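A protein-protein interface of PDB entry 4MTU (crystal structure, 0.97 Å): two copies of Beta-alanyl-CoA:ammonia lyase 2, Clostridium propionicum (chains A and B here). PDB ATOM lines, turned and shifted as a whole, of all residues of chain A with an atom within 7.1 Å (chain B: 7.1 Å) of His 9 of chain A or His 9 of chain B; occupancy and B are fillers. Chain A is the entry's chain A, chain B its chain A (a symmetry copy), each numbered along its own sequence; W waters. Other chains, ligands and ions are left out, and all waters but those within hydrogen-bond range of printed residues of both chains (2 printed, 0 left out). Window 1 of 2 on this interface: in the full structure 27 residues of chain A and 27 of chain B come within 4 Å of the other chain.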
ATOM      1  N   LYS A   4      39.709  10.676 -29.094  1.00  0.00           N
ATOM      2  CA  LYS A   4      38.479  10.353 -29.830  1.00  0.00           C
ATOM      3  C   LYS A   4      37.866  11.652 -30.339  1.00  0.00           C
ATOM      4  O   LYS A   4      38.045  12.714 -29.789  1.00  0.00           O
ATOM      5  CB  LYS A   4      37.471   9.638 -28.893  1.00  0.00           C
ATOM      6  CG  LYS A   4      36.720  10.431 -27.854  1.00  0.00           C
ATOM      7  CD  LYS A   4      35.875   9.617 -26.881  1.00  0.00           C
ATOM      8  CE  LYS A   4      35.180  10.389 -25.779  1.00  0.00           C
ATOM      9  NZ  LYS A   4      34.492   9.523 -24.727  1.00  0.00           N
ATOM     10  N   VAL A   6      34.722  13.979 -30.511  1.00  0.00           N
ATOM     11  CA  VAL A   6      33.576  14.319 -29.689  1.00  0.00           C
ATOM     12  C   VAL A   6      32.450  14.748 -30.649  1.00  0.00           C
ATOM     13  O   VAL A   6      32.643  15.501 -31.584  1.00  0.00           O
ATOM     14  CB  VAL A   6      33.901  15.418 -28.719  1.00  0.00           C
ATOM     15  CG1 VAL A   6      32.670  16.041 -28.099  1.00  0.00           C
ATOM     16  CG2 VAL A   6      34.831  14.843 -27.623  1.00  0.00           C
ATOM     17  N   VAL A   7      31.252  14.225 -30.363  1.00  0.00           N
ATOM     18  CA  VAL A   7      30.059  14.490 -31.178  1.00  0.00           C
ATOM     19  C   VAL A   7      28.948  15.019 -30.283  1.00  0.00           C
ATOM     20  O   VAL A   7      28.484  14.327 -29.393  1.00  0.00           O
ATOM     21  CB  VAL A   7      29.600  13.232 -31.889  1.00  0.00           C
ATOM     22  CG1 VAL A   7      28.292  13.427 -32.657  1.00  0.00           C
ATOM     23  CG2 VAL A   7      30.674  12.693 -32.831  1.00  0.00           C
ATOM     24  N   HIS A   8      28.587  16.282 -30.455  1.00  0.00           N
ATOM     25  CA  HIS A   8      27.378  16.818 -29.870  1.00  0.00           C
ATOM     26  C   HIS A   8      26.234  16.625 -30.877  1.00  0.00           C
ATOM     27  O   HIS A   8      26.466  16.609 -32.086  1.00  0.00           O
ATOM     28  CB  HIS A   8      27.561  18.284 -29.475  1.00  0.00           C
ATOM     29  CG  HIS A   8      28.441  18.500 -28.303  1.00  0.00           C
ATOM     30  ND1 HIS A   8      28.462  19.689 -27.601  1.00  0.00           N
ATOM     31  CD2 HIS A   8      29.354  17.648 -27.748  1.00  0.00           C
ATOM     32  CE1 HIS A   8      29.332  19.537 -26.629  1.00  0.00           C
ATOM     33  NE2 HIS A   8      29.921  18.328 -26.677  1.00  0.00           N
ATOM     34  N   HIS A   9      25.027  16.521 -30.360  1.00  0.00           N
ATOM     35  CA  HIS A   9      23.867  16.249 -31.184  1.00  0.00           C
ATOM     36  C   HIS A   9      22.682  16.803 -30.455  1.00  0.00           C
ATOM     37  O   HIS A   9      22.454  16.468 -29.290  1.00  0.00           O
ATOM     38  CB  HIS A   9      23.816  14.732 -31.449  1.00  0.00           C
ATOM     39  CG  HIS A   9      22.643  14.224 -32.256  1.00  0.00           C
ATOM     40  ND1 HIS A   9      22.791  13.394 -33.326  1.00  0.00           N
ATOM     41  CD2 HIS A   9      21.329  14.398 -32.153  1.00  0.00           C
ATOM     42  CE1 HIS A   9      21.542  13.088 -33.824  1.00  0.00           C
ATOM     43  NE2 HIS A   9      20.631  13.706 -33.085  1.00  0.00           N
ATOM     44  N   LEU A  10      21.832  17.561 -31.189  1.00  0.00           N
ATOM     45  CA  LEU A  10      20.671  18.177 -30.569  1.00  0.00           C
ATOM     46  C   LEU A  10      19.739  18.691 -31.697  1.00  0.00           C
ATOM     47  O   LEU A  10      20.044  18.536 -32.860  1.00  0.00           O
ATOM     48  CB  LEU A  10      21.098  19.208 -29.516  1.00  0.00           C
ATOM     49  CG  LEU A  10      22.151  20.207 -30.004  1.00  0.00           C
ATOM     50  CD1 LEU A  10      21.643  21.181 -31.032  1.00  0.00           C
ATOM     51  CD2 LEU A  10      22.600  21.048 -28.770  1.00  0.00           C
ATOM     52  N   MET A  11      18.640  19.294 -31.275  1.00  0.00           N
ATOM     53  CA  MET A  11      17.639  19.862 -32.189  1.00  0.00           C
ATOM     54  C   MET A  11      17.687  21.371 -32.144  1.00  0.00           C
ATOM     55  O   MET A  11      17.842  21.959 -31.065  1.00  0.00           O
ATOM     56  CB  MET A  11      16.229  19.383 -31.763  1.00  0.00           C
ATOM     57  CG  MET A  11      15.166  19.665 -32.796  1.00  0.00           C
ATOM     58  SD  MET A  11      13.498  19.242 -32.188  1.00  0.00           S
ATOM     59  CE  MET A  11      13.094  20.733 -31.327  1.00  0.00           C
ATOM     60  N   GLN A  32      28.115  25.995 -30.229  1.00  0.00           N
ATOM     61  CA  GLN A  32      28.235  24.572 -29.969  1.00  0.00           C
ATOM     62  C   GLN A  32      29.681  24.090 -30.092  1.00  0.00           C
ATOM     63  O   GLN A  32      30.116  23.268 -29.269  1.00  0.00           O
ATOM     64  CB  GLN A  32      27.310  23.732 -30.890  1.00  0.00           C
ATOM     65  CG  GLN A  32      26.970  22.434 -30.239  1.00  0.00           C
ATOM     66  CD  GLN A  32      26.171  22.601 -28.981  1.00  0.00           C
ATOM     67  OE1 GLN A  32      25.268  23.463 -28.920  1.00  0.00           O
ATOM     68  NE2 GLN A  32      26.455  21.835 -27.970  1.00  0.00           N
ATOM     69  N   VAL A  36      32.010  21.793 -27.621  1.00  0.00           N
ATOM     70  CA  VAL A  36      32.751  20.624 -28.080  1.00  0.00           C
ATOM     71  C   VAL A  36      34.227  20.761 -27.702  1.00  0.00           C
ATOM     72  O   VAL A  36      34.861  19.837 -27.193  1.00  0.00           O
ATOM     73  CB  VAL A  36      32.586  20.438 -29.620  1.00  0.00           C
ATOM     74  CG1 VAL A  36      33.485  19.338 -30.131  1.00  0.00           C
ATOM     75  CG2 VAL A  36      31.134  20.113 -29.957  1.00  0.00           C
ATOM     76  N   GLU A  39      34.822  20.154 -24.074  1.00  0.00           N
ATOM     77  CA  GLU A  39      34.805  18.737 -23.721  1.00  0.00           C
ATOM     78  C   GLU A  39      36.155  18.095 -24.064  1.00  0.00           C
ATOM     79  O   GLU A  39      36.721  17.303 -23.277  1.00  0.00           O
ATOM     80  CB  GLU A  39      33.656  18.033 -24.445  1.00  0.00           C
ATOM     81  CG  GLU A  39      33.354  16.677 -23.845  1.00  0.00           C
ATOM     82  CD  GLU A  39      32.153  15.964 -24.425  1.00  0.00           C
ATOM     83  OE1 GLU A  39      31.287  16.589 -25.030  1.00  0.00           O
ATOM     84  OE2 GLU A  39      32.054  14.718 -24.201  1.00  0.00           O
ATOM     85  N   TYR A  43      38.955  16.334 -21.436  1.00  0.00           N
ATOM     86  CA  TYR A  43      39.521  14.999 -21.624  1.00  0.00           C
ATOM     87  C   TYR A  43      41.045  14.961 -21.768  1.00  0.00           C
ATOM     88  O   TYR A  43      41.687  14.045 -21.287  1.00  0.00           O
ATOM     89  CB  TYR A  43      38.871  14.306 -22.827  1.00  0.00           C
ATOM     90  CG  TYR A  43      37.401  14.045 -22.681  1.00  0.00           C
ATOM     91  CD1 TYR A  43      36.758  13.943 -21.453  1.00  0.00           C
ATOM     92  CD2 TYR A  43      36.594  13.893 -23.815  1.00  0.00           C
ATOM     93  CE1 TYR A  43      35.412  13.719 -21.336  1.00  0.00           C
ATOM     94  CE2 TYR A  43      35.251  13.664 -23.687  1.00  0.00           C
ATOM     95  CZ  TYR A  43      34.640  13.569 -22.471  1.00  0.00           C
ATOM     96  OH  TYR A  43      33.286  13.377 -22.345  1.00  0.00           O
ATOM     97  N   PHE A  68      17.761  18.859 -37.038  1.00  0.00           N
ATOM     98  CA  PHE A  68      18.578  18.093 -36.076  1.00  0.00           C
ATOM     99  C   PHE A  68      20.004  18.170 -36.557  1.00  0.00           C
ATOM    100  O   PHE A  68      20.281  17.927 -37.734  1.00  0.00           O
ATOM    101  CB  PHE A  68      18.075  16.680 -35.932  1.00  0.00           C
ATOM    102  CG  PHE A  68      16.766  16.568 -35.180  1.00  0.00           C
ATOM    103  CD1 PHE A  68      15.541  16.793 -35.818  1.00  0.00           C
ATOM    104  CD2 PHE A  68      16.751  16.277 -33.819  1.00  0.00           C
ATOM    105  CE1 PHE A  68      14.356  16.682 -35.110  1.00  0.00           C
ATOM    106  CE2 PHE A  68      15.575  16.166 -33.130  1.00  0.00           C
ATOM    107  CZ  PHE A  68      14.360  16.345 -33.771  1.00  0.00           C
ATOM    108  N   MET A  69      20.904  18.515 -35.621  1.00  0.00           N
ATOM    109  CA  MET A  69      22.262  18.895 -35.945  1.00  0.00           C
ATOM    110  C   MET A  69      23.262  18.115 -35.101  1.00  0.00           C
ATOM    111  O   MET A  69      23.057  17.905 -33.910  1.00  0.00           O
ATOM    112  CB  MET A  69      22.463  20.385 -35.652  1.00  0.00           C
ATOM    113  CG  MET A  69      21.667  21.337 -36.544  1.00  0.00           C
ATOM    114  SD  MET A  69      22.136  21.340 -38.276  1.00  0.00           S
ATOM    115  CE  MET A  69      23.756  22.108 -38.108  1.00  0.00           C
ATOM    116  N   GLU A  70      24.360  17.762 -35.735  1.00  0.00           N
ATOM    117  CA  GLU A  70      25.513  17.184 -35.074  1.00  0.00           C
ATOM    118  C   GLU A  70      26.719  18.110 -35.235  1.00  0.00           C
ATOM    119  O   GLU A  70      26.905  18.791 -36.269  1.00  0.00           O
ATOM    120  CB  GLU A  70      25.900  15.860 -35.611  1.00  0.00           C
ATOM    121  CG  GLU A  70      24.965  14.835 -35.330  1.00  0.00           C
ATOM    122  CD  GLU A  70      25.503  13.406 -35.361  1.00  0.00           C
ATOM    123  OE1 GLU A  70      24.854  12.544 -34.803  1.00  0.00           O
ATOM    124  OE2 GLU A  70      26.572  13.139 -35.992  1.00  0.00           O
ATOM    125  N   TYR A  71      27.553  18.155 -34.212  1.00  0.00           N
ATOM    126  CA  TYR A  71      28.699  19.031 -34.152  1.00  0.00           C
ATOM    127  C   TYR A  71      29.873  18.141 -33.723  1.00  0.00           C
ATOM    128  O   TYR A  71      29.852  17.621 -32.629  1.00  0.00           O
ATOM    129  CB  TYR A  71      28.500  20.182 -33.190  1.00  0.00           C
ATOM    130  CG  TYR A  71      27.225  20.940 -33.466  1.00  0.00           C
ATOM    131  CD1 TYR A  71      27.245  22.097 -34.233  1.00  0.00           C
ATOM    132  CD2 TYR A  71      26.014  20.528 -32.972  1.00  0.00           C
ATOM    133  CE1 TYR A  71      26.074  22.806 -34.487  1.00  0.00           C
ATOM    134  CE2 TYR A  71      24.840  21.233 -33.224  1.00  0.00           C
ATOM    135  CZ  TYR A  71      24.865  22.369 -33.977  1.00  0.00           C
ATOM    136  OH  TYR A  71      23.687  23.028 -34.187  1.00  0.00           O
ATOM    137  N   VAL A  92      21.205  16.298 -39.890  1.00  0.00           N
ATOM    138  CA  VAL A  92      20.770  14.914 -39.973  1.00  0.00           C
ATOM    139  C   VAL A  92      19.271  14.741 -40.148  1.00  0.00           C
ATOM    140  O   VAL A  92      18.838  13.599 -40.466  1.00  0.00           O
ATOM    141  CB  VAL A  92      21.302  14.044 -38.784  1.00  0.00           C
ATOM    142  CG1 VAL A  92      22.819  14.147 -38.751  1.00  0.00           C
ATOM    143  CG2 VAL A  92      20.676  14.436 -37.485  1.00  0.00           C
ATOM    144  N   LYS B   4      17.212   2.397 -34.783  1.00  0.00           N
ATOM    145  CA  LYS B   4      18.454   2.694 -34.056  1.00  0.00           C
ATOM    146  C   LYS B   4      18.104   3.509 -32.816  1.00  0.00           C
ATOM    147  O   LYS B   4      17.123   4.210 -32.756  1.00  0.00           O
ATOM    148  CB  LYS B   4      19.415   3.512 -34.957  1.00  0.00           C
ATOM    149  CG  LYS B   4      19.141   4.972 -35.218  1.00  0.00           C
ATOM    150  CD  LYS B   4      20.048   5.646 -36.238  1.00  0.00           C
ATOM    151  CE  LYS B   4      19.735   7.090 -36.575  1.00  0.00           C
ATOM    152  NZ  LYS B   4      20.553   7.671 -37.724  1.00  0.00           N
ATOM    153  N   VAL B   6      18.709   6.757 -30.716  1.00  0.00           N
ATOM    154  CA  VAL B   6      19.069   8.145 -30.940  1.00  0.00           C
ATOM    155  C   VAL B   6      19.776   8.635 -29.662  1.00  0.00           C
ATOM    156  O   VAL B   6      19.349   8.397 -28.549  1.00  0.00           O
ATOM    157  CB  VAL B   6      17.861   8.984 -31.239  1.00  0.00           C
ATOM    158  CG1 VAL B   6      18.132  10.469 -31.130  1.00  0.00           C
ATOM    159  CG2 VAL B   6      17.356   8.626 -32.658  1.00  0.00           C
ATOM    160  N   VAL B   7      20.890   9.341 -29.884  1.00  0.00           N
ATOM    161  CA  VAL B   7      21.723   9.869 -28.796  1.00  0.00           C
ATOM    162  C   VAL B   7      21.911  11.366 -28.989  1.00  0.00           C
ATOM    163  O   VAL B   7      22.494  11.798 -29.969  1.00  0.00           O
ATOM    164  CB  VAL B   7      23.070   9.176 -28.759  1.00  0.00           C
ATOM    165  CG1 VAL B   7      24.018   9.772 -27.717  1.00  0.00           C
ATOM    166  CG2 VAL B   7      22.926   7.674 -28.523  1.00  0.00           C
ATOM    167  N   HIS B   8      21.333  12.165 -28.104  1.00  0.00           N
ATOM    168  CA  HIS B   8      21.657  13.571 -28.017  1.00  0.00           C
ATOM    169  C   HIS B   8      22.816  13.734 -27.021  1.00  0.00           C
ATOM    170  O   HIS B   8      22.954  12.937 -26.093  1.00  0.00           O
ATOM    171  CB  HIS B   8      20.431  14.396 -27.620  1.00  0.00           C
ATOM    172  CG  HIS B   8      19.400  14.512 -28.677  1.00  0.00           C
ATOM    173  ND1 HIS B   8      18.402  15.467 -28.637  1.00  0.00           N
ATOM    174  CD2 HIS B   8      19.226  13.742 -29.793  1.00  0.00           C
ATOM    175  CE1 HIS B   8      17.679  15.298 -29.720  1.00  0.00           C
ATOM    176  NE2 HIS B   8      18.115  14.257 -30.450  1.00  0.00           N
ATOM    177  N   HIS B   9      23.594  14.780 -27.212  1.00  0.00           N
ATOM    178  CA  HIS B   9      24.773  15.007 -26.403  1.00  0.00           C
ATOM    179  C   HIS B   9      25.034  16.483 -26.430  1.00  0.00           C
ATOM    180  O   HIS B   9      25.145  17.076 -27.506  1.00  0.00           O
ATOM    181  CB  HIS B   9      25.912  14.135 -26.964  1.00  0.00           C
ATOM    182  CG  HIS B   9      27.259  14.263 -26.290  1.00  0.00           C
ATOM    183  ND1 HIS B   9      27.981  13.182 -25.881  1.00  0.00           N
ATOM    184  CD2 HIS B   9      28.018  15.306 -25.971  1.00  0.00           C
ATOM    185  CE1 HIS B   9      29.168  13.625 -25.335  1.00  0.00           C
ATOM    186  NE2 HIS B   9      29.194  14.948 -25.402  1.00  0.00           N
ATOM    187  N   LEU B  10      25.273  17.067 -25.232  1.00  0.00           N
ATOM    188  CA  LEU B  10      25.500  18.500 -25.143  1.00  0.00           C
ATOM    189  C   LEU B  10      26.057  18.812 -23.729  1.00  0.00           C
ATOM    190  O   LEU B  10      26.230  17.918 -22.930  1.00  0.00           O
ATOM    191  CB  LEU B  10      24.250  19.279 -25.570  1.00  0.00           C
ATOM    192  CG  LEU B  10      22.956  18.808 -24.899  1.00  0.00           C
ATOM    193  CD1 LEU B  10      22.880  19.114 -23.429  1.00  0.00           C
ATOM    194  CD2 LEU B  10      21.777  19.570 -25.579  1.00  0.00           C
ATOM    195  N   MET B  11      26.298  20.092 -23.500  1.00  0.00           N
ATOM    196  CA  MET B  11      26.814  20.591 -22.217  1.00  0.00           C
ATOM    197  C   MET B  11      25.734  21.347 -21.478  1.00  0.00           C
ATOM    198  O   MET B  11      24.967  22.101 -22.093  1.00  0.00           O
ATOM    199  CB  MET B  11      28.010  21.537 -22.481  1.00  0.00           C
ATOM    200  CG  MET B  11      28.793  21.873 -21.236  1.00  0.00           C
ATOM    201  SD  MET B  11      30.084  23.118 -21.558  1.00  0.00           S
ATOM    202  CE  MET B  11      29.134  24.601 -21.390  1.00  0.00           C
ATOM    203  N   GLN B  32      14.937  17.532 -23.114  1.00  0.00           N
ATOM    204  CA  GLN B  32      15.769  16.863 -24.098  1.00  0.00           C
ATOM    205  C   GLN B  32      15.136  15.563 -24.592  1.00  0.00           C
ATOM    206  O   GLN B  32      15.204  15.276 -25.797  1.00  0.00           O
ATOM    207  CB  GLN B  32      17.201  16.592 -23.561  1.00  0.00           C
ATOM    208  CG  GLN B  32      18.170  16.507 -24.690  1.00  0.00           C
ATOM    209  CD  GLN B  32      18.306  17.796 -25.444  1.00  0.00           C
ATOM    210  OE1 GLN B  32      18.322  18.884 -24.831  1.00  0.00           O
ATOM    211  NE2 GLN B  32      18.397  17.739 -26.740  1.00  0.00           N
ATOM    212  N   VAL B  36      14.525  14.088 -28.367  1.00  0.00           N
ATOM    213  CA  VAL B  36      14.926  12.746 -28.775  1.00  0.00           C
ATOM    214  C   VAL B  36      13.729  12.000 -29.365  1.00  0.00           C
ATOM    215  O   VAL B  36      13.806  11.362 -30.414  1.00  0.00           O
ATOM    216  CB  VAL B  36      15.533  11.963 -27.571  1.00  0.00           C
ATOM    217  CG1 VAL B  36      15.792  10.522 -27.940  1.00  0.00           C
ATOM    218  CG2 VAL B  36      16.834  12.620 -27.120  1.00  0.00           C
ATOM    219  N   GLU B  39      12.875  13.175 -32.796  1.00  0.00           N
ATOM    220  CA  GLU B  39      13.774  12.653 -33.820  1.00  0.00           C
ATOM    221  C   GLU B  39      13.369  11.222 -34.194  1.00  0.00           C
ATOM    222  O   GLU B  39      13.336  10.842 -35.387  1.00  0.00           O
ATOM    223  CB  GLU B  39      15.219  12.707 -33.321  1.00  0.00           C
ATOM    224  CG  GLU B  39      16.216  12.539 -34.448  1.00  0.00           C
ATOM    225  CD  GLU B  39      17.668  12.699 -34.059  1.00  0.00           C
ATOM    226  OE1 GLU B  39      17.979  13.296 -33.032  1.00  0.00           O
ATOM    227  OE2 GLU B  39      18.538  12.253 -34.869  1.00  0.00           O
ATOM    228  N   TYR B  43      12.029   9.777 -37.932  1.00  0.00           N
ATOM    229  CA  TYR B  43      12.600   8.613 -38.607  1.00  0.00           C
ATOM    230  C   TYR B  43      11.613   7.474 -38.871  1.00  0.00           C
ATOM    231  O   TYR B  43      11.686   6.818 -39.896  1.00  0.00           O
ATOM    232  CB  TYR B  43      13.809   8.081 -37.828  1.00  0.00           C
ATOM    233  CG  TYR B  43      14.964   9.034 -37.735  1.00  0.00           C
ATOM    234  CD1 TYR B  43      15.184  10.064 -38.642  1.00  0.00           C
ATOM    235  CD2 TYR B  43      15.892   8.920 -36.693  1.00  0.00           C
ATOM    236  CE1 TYR B  43      16.235  10.935 -38.535  1.00  0.00           C
ATOM    237  CE2 TYR B  43      16.942   9.791 -36.599  1.00  0.00           C
ATOM    238  CZ  TYR B  43      17.138  10.797 -37.499  1.00  0.00           C
ATOM    239  OH  TYR B  43      18.171  11.695 -37.382  1.00  0.00           O
ATOM    240  N   PHE B  68      28.569  17.471 -18.794  1.00  0.00           N
ATOM    241  CA  PHE B  68      28.305  17.022 -20.176  1.00  0.00           C
ATOM    242  C   PHE B  68      27.386  15.833 -20.080  1.00  0.00           C
ATOM    243  O   PHE B  68      27.642  14.906 -19.308  1.00  0.00           O
ATOM    244  CB  PHE B  68      29.586  16.728 -20.912  1.00  0.00           C
ATOM    245  CG  PHE B  68      30.385  17.960 -21.275  1.00  0.00           C
ATOM    246  CD1 PHE B  68      31.223  18.583 -20.345  1.00  0.00           C
ATOM    247  CD2 PHE B  68      30.271  18.533 -22.539  1.00  0.00           C
ATOM    248  CE1 PHE B  68      31.946  19.709 -20.702  1.00  0.00           C
ATOM    249  CE2 PHE B  68      30.992  19.643 -22.883  1.00  0.00           C
ATOM    250  CZ  PHE B  68      31.857  20.234 -21.975  1.00  0.00           C
ATOM    251  N   MET B  69      26.308  15.878 -20.881  1.00  0.00           N
ATOM    252  CA  MET B  69      25.191  14.970 -20.740  1.00  0.00           C
ATOM    253  C   MET B  69      24.838  14.327 -22.076  1.00  0.00           C
ATOM    254  O   MET B  69      24.841  14.982 -23.113  1.00  0.00           O
ATOM    255  CB  MET B  69      23.960  15.740 -20.251  1.00  0.00           C
ATOM    256  CG  MET B  69      24.065  16.303 -18.835  1.00  0.00           C
ATOM    257  SD  MET B  69      24.152  15.080 -17.525  1.00  0.00           S
ATOM    258  CE  MET B  69      22.473  14.445 -17.647  1.00  0.00           C
ATOM    259  N   GLU B  70      24.476  13.064 -22.001  1.00  0.00           N
ATOM    260  CA  GLU B  70      23.924  12.324 -23.118  1.00  0.00           C
ATOM    261  C   GLU B  70      22.498  11.882 -22.790  1.00  0.00           C
ATOM    262  O   GLU B  70      22.147  11.561 -21.631  1.00  0.00           O
ATOM    263  CB  GLU B  70      24.693  11.107 -23.460  1.00  0.00           C
ATOM    264  CG  GLU B  70      25.972  11.376 -24.003  1.00  0.00           C
ATOM    265  CD  GLU B  70      26.591  10.266 -24.850  1.00  0.00           C
ATOM    266  OE1 GLU B  70      27.497  10.565 -25.603  1.00  0.00           O
ATOM    267  OE2 GLU B  70      26.190   9.068 -24.726  1.00  0.00           O
ATOM    268  N   TYR B  71      21.650  11.866 -23.802  1.00  0.00           N
ATOM    269  CA  TYR B  71      20.247  11.554 -23.667  1.00  0.00           C
ATOM    270  C   TYR B  71      19.949  10.521 -24.762  1.00  0.00           C
ATOM    271  O   TYR B  71      20.061  10.842 -25.925  1.00  0.00           O
ATOM    272  CB  TYR B  71      19.365  12.777 -23.808  1.00  0.00           C
ATOM    273  CG  TYR B  71      19.787  13.892 -22.884  1.00  0.00           C
ATOM    274  CD1 TYR B  71      19.162  14.065 -21.657  1.00  0.00           C
ATOM    275  CD2 TYR B  71      20.785  14.772 -23.216  1.00  0.00           C
ATOM    276  CE1 TYR B  71      19.539  15.096 -20.802  1.00  0.00           C
ATOM    277  CE2 TYR B  71      21.167  15.803 -22.364  1.00  0.00           C
ATOM    278  CZ  TYR B  71      20.550  15.970 -21.161  1.00  0.00           C
ATOM    279  OH  TYR B  71      20.957  17.003 -20.364  1.00  0.00           O
ATOM    280  N   VAL B  92      28.637  12.321 -18.609  1.00  0.00           N
ATOM    281  CA  VAL B  92      29.905  11.875 -19.160  1.00  0.00           C
ATOM    282  C   VAL B  92      31.095  12.725 -18.750  1.00  0.00           C
ATOM    283  O   VAL B  92      32.252  12.277 -18.982  1.00  0.00           O
ATOM    284  CB  VAL B  92      29.853  11.688 -20.714  1.00  0.00           C
ATOM    285  CG1 VAL B  92      28.732  10.716 -21.047  1.00  0.00           C
ATOM    286  CG2 VAL B  92      29.707  12.994 -21.426  1.00  0.00           C
HETATM  287  O   HOH W   1      17.795  19.767 -28.568  1.00  0.00           O
HETATM  288  O   HOH W   2      25.911  22.323 -25.272  1.00  0.00           O
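The backbone NH (N) of His 9 of chain A is in hydrogen-bond range of the backbone carbonyl oxygen (O) of His 9 of chain B (2.9 Å).
A ring nitrogen (NE2) of His 9 of chain A lies within hydrogen-bond range of the side-chain carboxylate of Glu 39 of chain B (2.7 Å).
NE2 of His 9 of chain B is in hydrogen-bond range of OE1 of Glu 39 of chain A (2.7 Å).
O of His 8 of chain A sits at hydrogen-bond distance from N of Tyr 71 of chain A (2.8 Å).
The backbone carbonyl oxygen (O) of Leu 10 of chain A lies within hydrogen-bond range of the backbone NH (N) of Met 69 of chain A.
A ring nitrogen (ND1) of His 8 of chain B sits at hydrogen-bond distance from the side-chain amide nitrogen (NE2) of Gln 32 of chain B (3.0 Å).
NE2 of His 8 of chain B is in hydrogen-bond range of OE1 of Glu 39 of chain B, 2.8 Å away.
O of His 8 of chain B is in hydrogen-bond range of N of Tyr 71 of chain B, at 2.8 Å.
OE2 of Glu 39 of chain B is in hydrogen-bond range of OH of Tyr 43 of chain B, at 2.6 Å.
Among the printed residues, pairs that only touch across the chains: Val 7 of chain A with His 9 of chain B (3.3 Å), His 8 of chain A with His 9 of chain B (3.2 Å), His 9 of chain A with Val 7 of chain B (3.3 Å), His 9 of chain A with His 8 of chain B (3.2 Å), Leu 10 of chain A with Leu 10 of chain B (3.6 Å), Glu 39 of chain A with Phe 68 of chain B (3.3 Å), Tyr 43 of chain A with Val 92 of chain B (3.7 Å), Phe 68 of chain A with Glu 39 of chain B (3.3 Å) and Val 92 of chain A with Tyr 43 of chain B (3.7 Å).
Of the printed residues of chain B, His 9 of chain A touches Val 7, His 8, His 9 and Glu 39.
Printed residues of chain A within 4 Å of His 9 of chain B: Val 7 (3.3 Å), His 8 (3.2 Å), His 9 (2.9 Å) and Glu 39 (2.7 Å).
Printed residues of chain B within 4 Å of Glu 39 of chain A: His 9 (2.7 Å) and Phe 68 (3.3 Å).
Of the printed residues of chain B, Tyr 43 of chain A touches Val 92.
Of the printed residues of chain A, Leu 10 of chain B touches Leu 10 (3.6 Å).
Printed residues of chain A within 4 Å of Val 92 of chain B: Tyr 43.
Gln 32 of chain A touches none of the printed residues of chain B.
Met 11 of chain B touches none of the printed residues of chain A.
Of the 16 printed residues of chain A, 8 touch a printed residue of chain B.
Printed residues of chain A that touch a printed residue of chain B: Val 7, His 8, His 9, Leu 10, Glu 39, Tyr 43, Phe 68 and Val 92.
Hydrophobic or aromatic side chains of chain A within 4 Å of the printed part of chain B: His 8, His 9, Leu 10, Tyr 43, Phe 68 and Val 92.
Printed residues of chain B that touch a printed residue of chain A: Val 7, His 8, His 9, Leu 10, Glu 39, Tyr 43, Phe 68 and Val 92.
Among the printed residues, 12 pairs touch across the chains.
Among the printed residues, no Asp or Glu carboxylate lies within 4 Å of a Lys or Arg side-chain nitrogen of the other chain.
His 9 of chain B touches its own counterpart, His 9 of chain A.
His 9 of chain A touches Glu 39 of chain B, and with the chains exchanged Glu 39 of chain A touches His 9 of chain B.
Leu 10 of chain B touches its own counterpart, Leu 10 of chain A.
Glu 39 of chain A touches Phe 68 of chain B, and with the chains exchanged Phe 68 of chain A touches Glu 39 of chain B.
Positions printed for both chains: 4, 6, 7, 8, 9, 10, 11, 32, 36, 39, 43, 68, 69, 70, 71 and 92.
Of the 12 pairs that touch across the chains among the printed residues, 12 have their exchanged pair printed and touching as well.
Water W2 bridges NE2 of Gln 32 of chain A and N of Met 11 of chain B.
Water W1 bridges the side-chain amide nitrogen (NE2) of Gln 32 of chain B and the backbone NH (N) of Met 11 of chain A.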
